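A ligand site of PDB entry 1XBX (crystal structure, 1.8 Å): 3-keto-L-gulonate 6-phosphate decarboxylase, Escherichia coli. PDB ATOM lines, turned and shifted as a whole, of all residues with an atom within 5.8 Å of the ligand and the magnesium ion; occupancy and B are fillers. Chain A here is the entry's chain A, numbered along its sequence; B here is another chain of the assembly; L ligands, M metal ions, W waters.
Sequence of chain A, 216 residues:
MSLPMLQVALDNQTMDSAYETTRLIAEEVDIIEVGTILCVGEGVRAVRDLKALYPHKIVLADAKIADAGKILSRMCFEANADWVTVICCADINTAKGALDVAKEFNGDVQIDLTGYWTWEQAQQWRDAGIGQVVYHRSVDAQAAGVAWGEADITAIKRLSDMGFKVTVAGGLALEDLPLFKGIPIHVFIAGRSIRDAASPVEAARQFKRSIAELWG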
ATOM      1  N   ALA A   9     -24.733   5.280  -6.384  1.00  0.00           N
ATOM      2  CA  ALA A   9     -24.309   5.295  -7.778  1.00  0.00           C
ATOM      3  C   ALA A   9     -25.539   5.492  -8.606  1.00  0.00           C
ATOM      4  O   ALA A   9     -26.465   4.712  -8.519  1.00  0.00           O
ATOM      5  CB  ALA A   9     -23.651   3.994  -8.164  1.00  0.00           C
ATOM      6  N   ASP A  11     -26.506   4.909 -11.897  1.00  0.00           N
ATOM      7  CA  ASP A  11     -26.226   4.195 -13.151  1.00  0.00           C
ATOM      8  C   ASP A  11     -27.437   4.216 -14.056  1.00  0.00           C
ATOM      9  O   ASP A  11     -27.888   3.213 -14.523  1.00  0.00           O
ATOM     10  CB  ASP A  11     -25.712   2.782 -12.854  1.00  0.00           C
ATOM     11  CG  ASP A  11     -24.303   2.795 -12.297  1.00  0.00           C
ATOM     12  OD1 ASP A  11     -23.462   3.561 -12.915  1.00  0.00           O
ATOM     13  OD2 ASP A  11     -23.972   2.159 -11.254  1.00  0.00           O
ATOM     14  N   GLU A  33     -22.754   9.688  -6.917  1.00  0.00           N
ATOM     15  CA  GLU A  33     -21.957   9.278  -8.063  1.00  0.00           C
ATOM     16  C   GLU A  33     -22.751   9.405  -9.358  1.00  0.00           C
ATOM     17  O   GLU A  33     -23.856   8.863  -9.523  1.00  0.00           O
ATOM     18  CB  GLU A  33     -21.421   7.860  -7.895  1.00  0.00           C
ATOM     19  CG  GLU A  33     -21.049   7.169  -9.197  1.00  0.00           C
ATOM     20  CD  GLU A  33     -20.691   5.702  -9.075  1.00  0.00           C
ATOM     21  OE1 GLU A  33     -20.332   5.287  -7.981  1.00  0.00           O
ATOM     22  OE2 GLU A  33     -20.783   4.960 -10.104  1.00  0.00           O
ATOM     23  N   VAL A  34     -22.143  10.107 -10.301  1.00  0.00           N
ATOM     24  CA  VAL A  34     -22.553  10.066 -11.651  1.00  0.00           C
ATOM     25  C   VAL A  34     -21.953   8.794 -12.244  1.00  0.00           C
ATOM     26  O   VAL A  34     -20.764   8.720 -12.532  1.00  0.00           O
ATOM     27  CB  VAL A  34     -22.042  11.276 -12.409  1.00  0.00           C
ATOM     28  CG1 VAL A  34     -22.566  11.230 -13.831  1.00  0.00           C
ATOM     29  CG2 VAL A  34     -22.518  12.534 -11.754  1.00  0.00           C
ATOM     30  N   GLY A  35     -22.782   7.755 -12.366  1.00  0.00           N
ATOM     31  CA  GLY A  35     -22.270   6.485 -12.799  1.00  0.00           C
ATOM     32  C   GLY A  35     -21.696   6.508 -14.161  1.00  0.00           C
ATOM     33  O   GLY A  35     -22.003   7.378 -15.000  1.00  0.00           O
ATOM     34  N   THR A  36     -20.872   5.521 -14.488  1.00  0.00           N
ATOM     35  CA  THR A  36     -20.377   5.410 -15.847  1.00  0.00           C
ATOM     36  C   THR A  36     -21.470   5.396 -16.888  1.00  0.00           C
ATOM     37  O   THR A  36     -21.353   6.020 -17.957  1.00  0.00           O
ATOM     38  CB  THR A  36     -19.494   4.174 -16.010  1.00  0.00           C
ATOM     39  OG1 THR A  36     -18.601   4.080 -14.898  1.00  0.00           O
ATOM     40  CG2 THR A  36     -18.588   4.340 -17.265  1.00  0.00           C
ATOM     41  N   ASP A  62     -17.841   8.907 -12.305  1.00  0.00           N
ATOM     42  CA  ASP A  62     -17.264   7.595 -12.426  1.00  0.00           C
ATOM     43  C   ASP A  62     -16.909   7.333 -13.889  1.00  0.00           C
ATOM     44  O   ASP A  62     -17.404   6.394 -14.542  1.00  0.00           O
ATOM     45  CB  ASP A  62     -18.199   6.532 -11.862  1.00  0.00           C
ATOM     46  CG  ASP A  62     -17.516   5.201 -11.635  1.00  0.00           C
ATOM     47  OD1 ASP A  62     -16.259   5.156 -11.641  1.00  0.00           O
ATOM     48  OD2 ASP A  62     -18.188   4.157 -11.497  1.00  0.00           O
ATOM     49  N   LYS A  64     -13.944   6.356 -15.117  1.00  0.00           N
ATOM     50  CA  LYS A  64     -13.105   5.180 -15.316  1.00  0.00           C
ATOM     51  C   LYS A  64     -12.103   5.487 -16.428  1.00  0.00           C
ATOM     52  O   LYS A  64     -11.933   4.726 -17.380  1.00  0.00           O
ATOM     53  CB  LYS A  64     -13.956   3.901 -15.556  1.00  0.00           C
ATOM     54  CG  LYS A  64     -14.697   3.506 -14.228  1.00  0.00           C
ATOM     55  CD  LYS A  64     -15.526   2.200 -14.371  1.00  0.00           C
ATOM     56  CE  LYS A  64     -16.501   2.013 -13.173  1.00  0.00           C
ATOM     57  NZ  LYS A  64     -17.582   0.986 -13.508  1.00  0.00           N
ATOM     58  N   HIS A 136     -13.459  -3.140  -6.194  1.00  0.00           N
ATOM     59  CA  HIS A 136     -14.675  -3.180  -6.981  1.00  0.00           C
ATOM     60  C   HIS A 136     -14.867  -4.528  -7.611  1.00  0.00           C
ATOM     61  O   HIS A 136     -14.058  -4.940  -8.477  1.00  0.00           O
ATOM     62  CB  HIS A 136     -14.572  -2.103  -8.086  1.00  0.00           C
ATOM     63  CG  HIS A 136     -15.903  -1.661  -8.622  1.00  0.00           C
ATOM     64  ND1 HIS A 136     -16.104  -0.377  -9.115  1.00  0.00           N
ATOM     65  CD2 HIS A 136     -17.096  -2.291  -8.706  1.00  0.00           C
ATOM     66  CE1 HIS A 136     -17.366  -0.250  -9.476  1.00  0.00           C
ATOM     67  NE2 HIS A 136     -17.988  -1.405  -9.275  1.00  0.00           N
ATOM     68  N   ARG A 137     -15.885  -5.276  -7.165  1.00  0.00           N
ATOM     69  CA  ARG A 137     -16.261  -6.465  -7.837  1.00  0.00           C
ATOM     70  C   ARG A 137     -16.976  -6.139  -9.124  1.00  0.00           C
ATOM     71  O   ARG A 137     -17.976  -5.389  -9.119  1.00  0.00           O
ATOM     72  CB  ARG A 137     -17.165  -7.349  -6.970  1.00  0.00           C
ATOM     73  CG  ARG A 137     -17.621  -8.594  -7.677  1.00  0.00           C
ATOM     74  CD  ARG A 137     -18.598  -9.480  -6.879  1.00  0.00           C
ATOM     75  NE  ARG A 137     -19.763  -8.746  -6.426  1.00  0.00           N
ATOM     76  CZ  ARG A 137     -20.833  -9.286  -5.850  1.00  0.00           C
ATOM     77  NH1 ARG A 137     -20.904 -10.598  -5.620  1.00  0.00           N
ATOM     78  NH2 ARG A 137     -21.827  -8.502  -5.451  1.00  0.00           N
ATOM     79  N   VAL A 139     -19.442  -5.962 -11.964  1.00  0.00           N
ATOM     80  CA  VAL A 139     -20.852  -6.336 -12.026  1.00  0.00           C
ATOM     81  C   VAL A 139     -21.127  -7.466 -13.013  1.00  0.00           C
ATOM     82  O   VAL A 139     -22.042  -8.275 -12.837  1.00  0.00           O
ATOM     83  CB  VAL A 139     -21.762  -5.134 -12.287  1.00  0.00           C
ATOM     84  CG1 VAL A 139     -21.462  -4.041 -11.290  1.00  0.00           C
ATOM     85  CG2 VAL A 139     -21.622  -4.634 -13.697  1.00  0.00           C
ATOM     86  N   GLN A 142     -19.954 -10.570 -11.135  1.00  0.00           N
ATOM     87  CA  GLN A 142     -21.092 -10.819 -10.236  1.00  0.00           C
ATOM     88  C   GLN A 142     -22.214 -11.610 -10.944  1.00  0.00           C
ATOM     89  O   GLN A 142     -22.711 -12.600 -10.386  1.00  0.00           O
ATOM     90  CB  GLN A 142     -21.596  -9.514  -9.625  1.00  0.00           C
ATOM     91  CG  GLN A 142     -22.900  -9.664  -8.820  1.00  0.00           C
ATOM     92  CD  GLN A 142     -23.571  -8.348  -8.518  1.00  0.00           C
ATOM     93  OE1 GLN A 142     -23.018  -7.284  -8.824  1.00  0.00           O
ATOM     94  NE2 GLN A 142     -24.758  -8.400  -7.898  1.00  0.00           N
ATOM     95  N   ALA A 169     -17.160  -1.453  -3.510  1.00  0.00           N
ATOM     96  CA  ALA A 169     -18.271  -1.433  -4.446  1.00  0.00           C
ATOM     97  C   ALA A 169     -18.453  -2.728  -5.174  1.00  0.00           C
ATOM     98  O   ALA A 169     -17.462  -3.478  -5.403  1.00  0.00           O
ATOM     99  CB  ALA A 169     -18.057  -0.324  -5.467  1.00  0.00           C
ATOM    100  N   GLY A 170     -19.666  -2.943  -5.659  1.00  0.00           N
ATOM    101  CA  GLY A 170     -19.974  -4.022  -6.560  1.00  0.00           C
ATOM    102  C   GLY A 170     -21.122  -4.870  -6.059  1.00  0.00           C
ATOM    103  O   GLY A 170     -20.924  -5.799  -5.251  1.00  0.00           O
ATOM    104  N   GLY A 171     -22.331  -4.503  -6.493  1.00  0.00           N
ATOM    105  CA  GLY A 171     -23.570  -5.157  -6.074  1.00  0.00           C
ATOM    106  C   GLY A 171     -23.762  -5.302  -4.588  1.00  0.00           C
ATOM    107  O   GLY A 171     -24.403  -6.286  -4.159  1.00  0.00           O
ATOM    108  N   LEU A 172     -23.288  -4.347  -3.797  1.00  0.00           N
ATOM    109  CA  LEU A 172     -23.421  -4.445  -2.329  1.00  0.00           C
ATOM    110  C   LEU A 172     -24.891  -4.385  -1.887  1.00  0.00           C
ATOM    111  O   LEU A 172     -25.671  -3.553  -2.357  1.00  0.00           O
ATOM    112  CB  LEU A 172     -22.620  -3.388  -1.603  1.00  0.00           C
ATOM    113  CG  LEU A 172     -21.086  -3.509  -1.642  1.00  0.00           C
ATOM    114  CD1 LEU A 172     -20.415  -2.382  -0.956  1.00  0.00           C
ATOM    115  CD2 LEU A 172     -20.606  -4.860  -1.050  1.00  0.00           C
ATOM    116  N   ILE A 189     -20.190   2.026  -1.683  1.00  0.00           N
ATOM    117  CA  ILE A 189     -21.099   2.401  -2.779  1.00  0.00           C
ATOM    118  C   ILE A 189     -22.260   1.421  -2.874  1.00  0.00           C
ATOM    119  O   ILE A 189     -22.051   0.209  -2.814  1.00  0.00           O
ATOM    120  CB  ILE A 189     -20.381   2.361  -4.122  1.00  0.00           C
ATOM    121  CG1 ILE A 189     -19.127   3.225  -4.061  1.00  0.00           C
ATOM    122  CG2 ILE A 189     -21.324   2.859  -5.208  1.00  0.00           C
ATOM    123  CD1 ILE A 189     -18.388   3.372  -5.423  1.00  0.00           C
ATOM    124  N   ALA A 190     -23.465   1.966  -3.078  1.00  0.00           N
ATOM    125  CA  ALA A 190     -24.641   1.186  -3.415  1.00  0.00           C
ATOM    126  C   ALA A 190     -25.336   1.848  -4.589  1.00  0.00           C
ATOM    127  O   ALA A 190     -25.663   3.029  -4.511  1.00  0.00           O
ATOM    128  CB  ALA A 190     -25.584   1.115  -2.261  1.00  0.00           C
ATOM    129  N   GLY A 191     -25.558   1.068  -5.660  1.00  0.00           N
ATOM    130  CA  GLY A 191     -26.336   1.503  -6.819  1.00  0.00           C
ATOM    131  C   GLY A 191     -27.676   0.801  -6.779  1.00  0.00           C
ATOM    132  O   GLY A 191     -28.658   1.316  -6.243  1.00  0.00           O
ATOM    133  N   ARG A 192     -27.690  -0.420  -7.278  1.00  0.00           N
ATOM    134  CA  ARG A 192     -28.932  -1.162  -7.454  1.00  0.00           C
ATOM    135  C   ARG A 192     -29.721  -1.362  -6.147  1.00  0.00           C
ATOM    136  O   ARG A 192     -30.950  -1.275  -6.139  1.00  0.00           O
ATOM    137  CB  ARG A 192     -28.655  -2.496  -8.133  1.00  0.00           C
ATOM    138  CG  ARG A 192     -28.408  -2.364  -9.597  1.00  0.00           C
ATOM    139  CD  ARG A 192     -27.759  -3.602 -10.182  1.00  0.00           C
ATOM    140  NE  ARG A 192     -26.367  -3.739  -9.744  1.00  0.00           N
ATOM    141  CZ  ARG A 192     -25.624  -4.822  -9.912  1.00  0.00           C
ATOM    142  NH1 ARG A 192     -24.390  -4.813  -9.502  1.00  0.00           N
ATOM    143  NH2 ARG A 192     -26.142  -5.936 -10.472  1.00  0.00           N
ATOM    144  N   SER A 193     -29.014  -1.622  -5.072  1.00  0.00           N
ATOM    145  CA  SER A 193     -29.659  -1.956  -3.793  1.00  0.00           C
ATOM    146  C   SER A 193     -30.350  -0.714  -3.188  1.00  0.00           C
ATOM    147  O   SER A 193     -31.245  -0.875  -2.318  1.00  0.00           O
ATOM    148  CB  SER A 193     -28.672  -2.618  -2.824  1.00  0.00           C
ATOM    149  OG  SER A 193     -27.712  -1.653  -2.391  1.00  0.00           O
ATOM    150  N   ARG A 195     -31.367   2.207  -5.682  1.00  0.00           N
ATOM    151  CA  ARG A 195     -32.267   2.625  -6.764  1.00  0.00           C
ATOM    152  C   ARG A 195     -33.447   1.705  -6.929  1.00  0.00           C
ATOM    153  O   ARG A 195     -34.548   2.171  -7.205  1.00  0.00           O
ATOM    154  CB  ARG A 195     -31.538   2.640  -8.097  1.00  0.00           C
ATOM    155  CG  ARG A 195     -30.352   3.655  -8.080  1.00  0.00           C
ATOM    156  CD  ARG A 195     -29.889   4.076  -9.514  1.00  0.00           C
ATOM    157  NE  ARG A 195     -29.884   2.900 -10.370  1.00  0.00           N
ATOM    158  CZ  ARG A 195     -28.885   2.016 -10.448  1.00  0.00           C
ATOM    159  NH1 ARG A 195     -27.773   2.217  -9.792  1.00  0.00           N
ATOM    160  NH2 ARG A 195     -29.005   0.947 -11.222  1.00  0.00           N
ATOM    161  N   ASP B  67     -16.535  -2.273 -17.458  1.00  0.00           N
ATOM    162  CA  ASP B  67     -17.474  -3.152 -16.728  1.00  0.00           C
ATOM    163  C   ASP B  67     -18.859  -2.762 -17.240  1.00  0.00           C
ATOM    164  O   ASP B  67     -19.018  -1.765 -17.957  1.00  0.00           O
ATOM    165  CB  ASP B  67     -17.334  -2.916 -15.233  1.00  0.00           C
ATOM    166  CG  ASP B  67     -17.994  -4.016 -14.372  1.00  0.00           C
ATOM    167  OD1 ASP B  67     -18.327  -5.091 -14.930  1.00  0.00           O
ATOM    168  OD2 ASP B  67     -18.189  -3.815 -13.160  1.00  0.00           O
ATOM    169  N   ALA B  68     -19.869  -3.526 -16.876  1.00  0.00           N
ATOM    170  CA  ALA B  68     -21.208  -3.357 -17.370  1.00  0.00           C
ATOM    171  C   ALA B  68     -21.263  -3.460 -18.889  1.00  0.00           C
ATOM    172  O   ALA B  68     -21.877  -2.630 -19.595  1.00  0.00           O
ATOM    173  CB  ALA B  68     -21.784  -2.068 -16.888  1.00  0.00           C
HETATM  174  O1  LIG L   1     -25.321  -1.449  -8.577  1.00  0.00           O
HETATM  175  P1  LIG L   1     -24.026  -1.394  -7.805  1.00  0.00           P
HETATM  176  O2  LIG L   1     -24.099  -1.296  -6.301  1.00  0.00           O
HETATM  177  O3  LIG L   1     -23.114  -2.478  -8.300  1.00  0.00           O
HETATM  178  O4  LIG L   1     -23.355  -0.010  -8.333  1.00  0.00           O
HETATM  179  C1  LIG L   1     -22.137   0.513  -7.856  1.00  0.00           C
HETATM  180  C2  LIG L   1     -21.019   0.174  -8.829  1.00  0.00           C
HETATM  181  O5  LIG L   1     -20.769  -1.237  -8.898  1.00  0.00           O
HETATM  182  C3  LIG L   1     -21.353   0.708 -10.204  1.00  0.00           C
HETATM  183  O6  LIG L   1     -21.609   2.115 -10.150  1.00  0.00           O
HETATM  184  C4  LIG L   1     -20.198   0.508 -11.160  1.00  0.00           C
HETATM  185  C5  LIG L   1     -20.031  -0.677 -11.886  1.00  0.00           C
HETATM  186 MG    MG M   1     -19.925   3.310 -10.765  1.00  0.00          MG
HETATM  187  O   HOH W   1     -22.155  -1.822  -4.739  1.00  0.00           O
HETATM  188  O   HOH W   2     -20.731   1.327 -14.645  1.00  0.00           O
HETATM  189  O   HOH W   3     -22.509  -0.685 -13.608  1.00  0.00           O
HETATM  190  O   HOH W   4     -16.789  -1.551 -12.328  1.00  0.00           O
HETATM  191  O   HOH W   5     -20.872   3.371 -12.646  1.00  0.00           O
HETATM  192  O   HOH W   6     -25.764   0.464 -10.446  1.00  0.00           O
HETATM  193  O   HOH W   7     -26.165  -2.624  -5.055  1.00  0.00           O
HETATM  194  O   HOH W   8     -18.976   3.066  -8.863  1.00  0.00           O
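The magnesium ion is bound by the side-chain carboxylate (OE2) of Glu 33 (2.0 Å).
OD2 of Asp 62 binds the magnesium ion (2.1 Å).
Water W5 binds the magnesium ion (2.1 Å).
Water W8 is bound to the magnesium ion.
O6 of the ligand is bound to the magnesium ion (2.2 Å).
The magnesium ion has five donor atoms within binding distance.
Water W5 bridges the side-chain carboxylate (OD1) of Asp 11 (2.6 Å) and the backbone NH (N) of Thr 36 (2.8 Å).
Water W6 lies within hydrogen-bond range of the side-chain carboxylate (OD2) of Asp 11 (2.6 Å), an oxygen (O1) of the ligand (2.7 Å) and the guanidinium group (NH1) of Arg 195 (2.7 Å).
Water W7 lies within hydrogen-bond range of O2 of the ligand (2.8 Å), O of Leu 172 (2.9 Å), N of Ser 193 (3.0 Å) and N of Arg 192 (3.5 Å).
Water W4 lies within hydrogen-bond range of OD2 of Asp 67 of chain B, NZ of Lys 64 and NE2 of His 136.
Water W2 bridges NZ of Lys 64 (3.4 Å) and OG1 of Thr 36 (3.5 Å).
OD2 of Asp 11 sits close to O6 of the ligand, 2.6 Å away.
N of Arg 192 lies within hydrogen-bond range of O1 of the ligand.
The guanidinium group (NE) of Arg 192 is in salt-bridge range of an oxygen (O1) of the ligand.
O5 of the ligand is in hydrogen-bond range of NE2 of His 136 (2.8 Å).
N of Gly 171 sits at hydrogen-bond distance from O3 of the ligand.
The backbone NH (N) of Gly 191 is in hydrogen-bond range of an oxygen (O2) of the ligand, 2.9 Å away.
OD2 of Asp 62 lies close to NZ of Lys 64, at 3.8 Å.
The backbone carbonyl oxygen (O) of Asp 62 lies within hydrogen-bond range of the side-chain hydroxyl (OG1) of Thr 36 (2.6 Å).
N of Asp 62 is in hydrogen-bond range of O of Val 34 (2.9 Å).
NH1 of Arg 192 sits at hydrogen-bond distance from OE1 of Gln 142.
N of Ala 9 is in hydrogen-bond range of O of Ala 190 (3.1 Å).
NH1 of Arg 195 lies within hydrogen-bond range of O of Ala 9 (3.1 Å).
The backbone NH (N) of Val 139 lies within hydrogen-bond range of the side-chain carboxylate (OD2) of Asp 67 of chain B (2.8 Å).
The backbone carbonyl oxygen of Gly 170 is in hydrogen-bond range of the guanidinium group of Arg 137, 2.9 Å away.
Two residues have an atom within 4 Å of the magnesium ion: Glu 33 and Asp 62.
The nearest printed residue that does not touch the magnesium ion is Asp 11 (4.1 Å).
Ala 9 touches the ligand (CB to O6, 3.4 Å).
NZ of Lys 64 touches C5 of the ligand, 3.4 Å away.
CG1 of Val 139 touches C5 of the ligand, 3.7 Å away.
Gly 170 touches the ligand.
Ile 189 touches the ligand (CG2 to C1, 3.6 Å).
C of Ala 190 touches O2 of the ligand (3.8 Å).
Asp 67 of chain B touches the ligand (OD2 to C5, 3.9 Å).
Hydrophobic or aromatic side chains that line the ligand: Ala 9, His 136, Val 139 and Ile 189.
Within 4 Å of the ligand: Ala 9, Asp 11, Glu 33, Lys 64, His 136, Val 139, Gly 170, Gly 171, Ile 189, Ala 190, Gly 191, Arg 192 and Asp 67 of chain B.
The nearest printed residue that does not touch the ligand is Leu 172 (4.03 Å).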
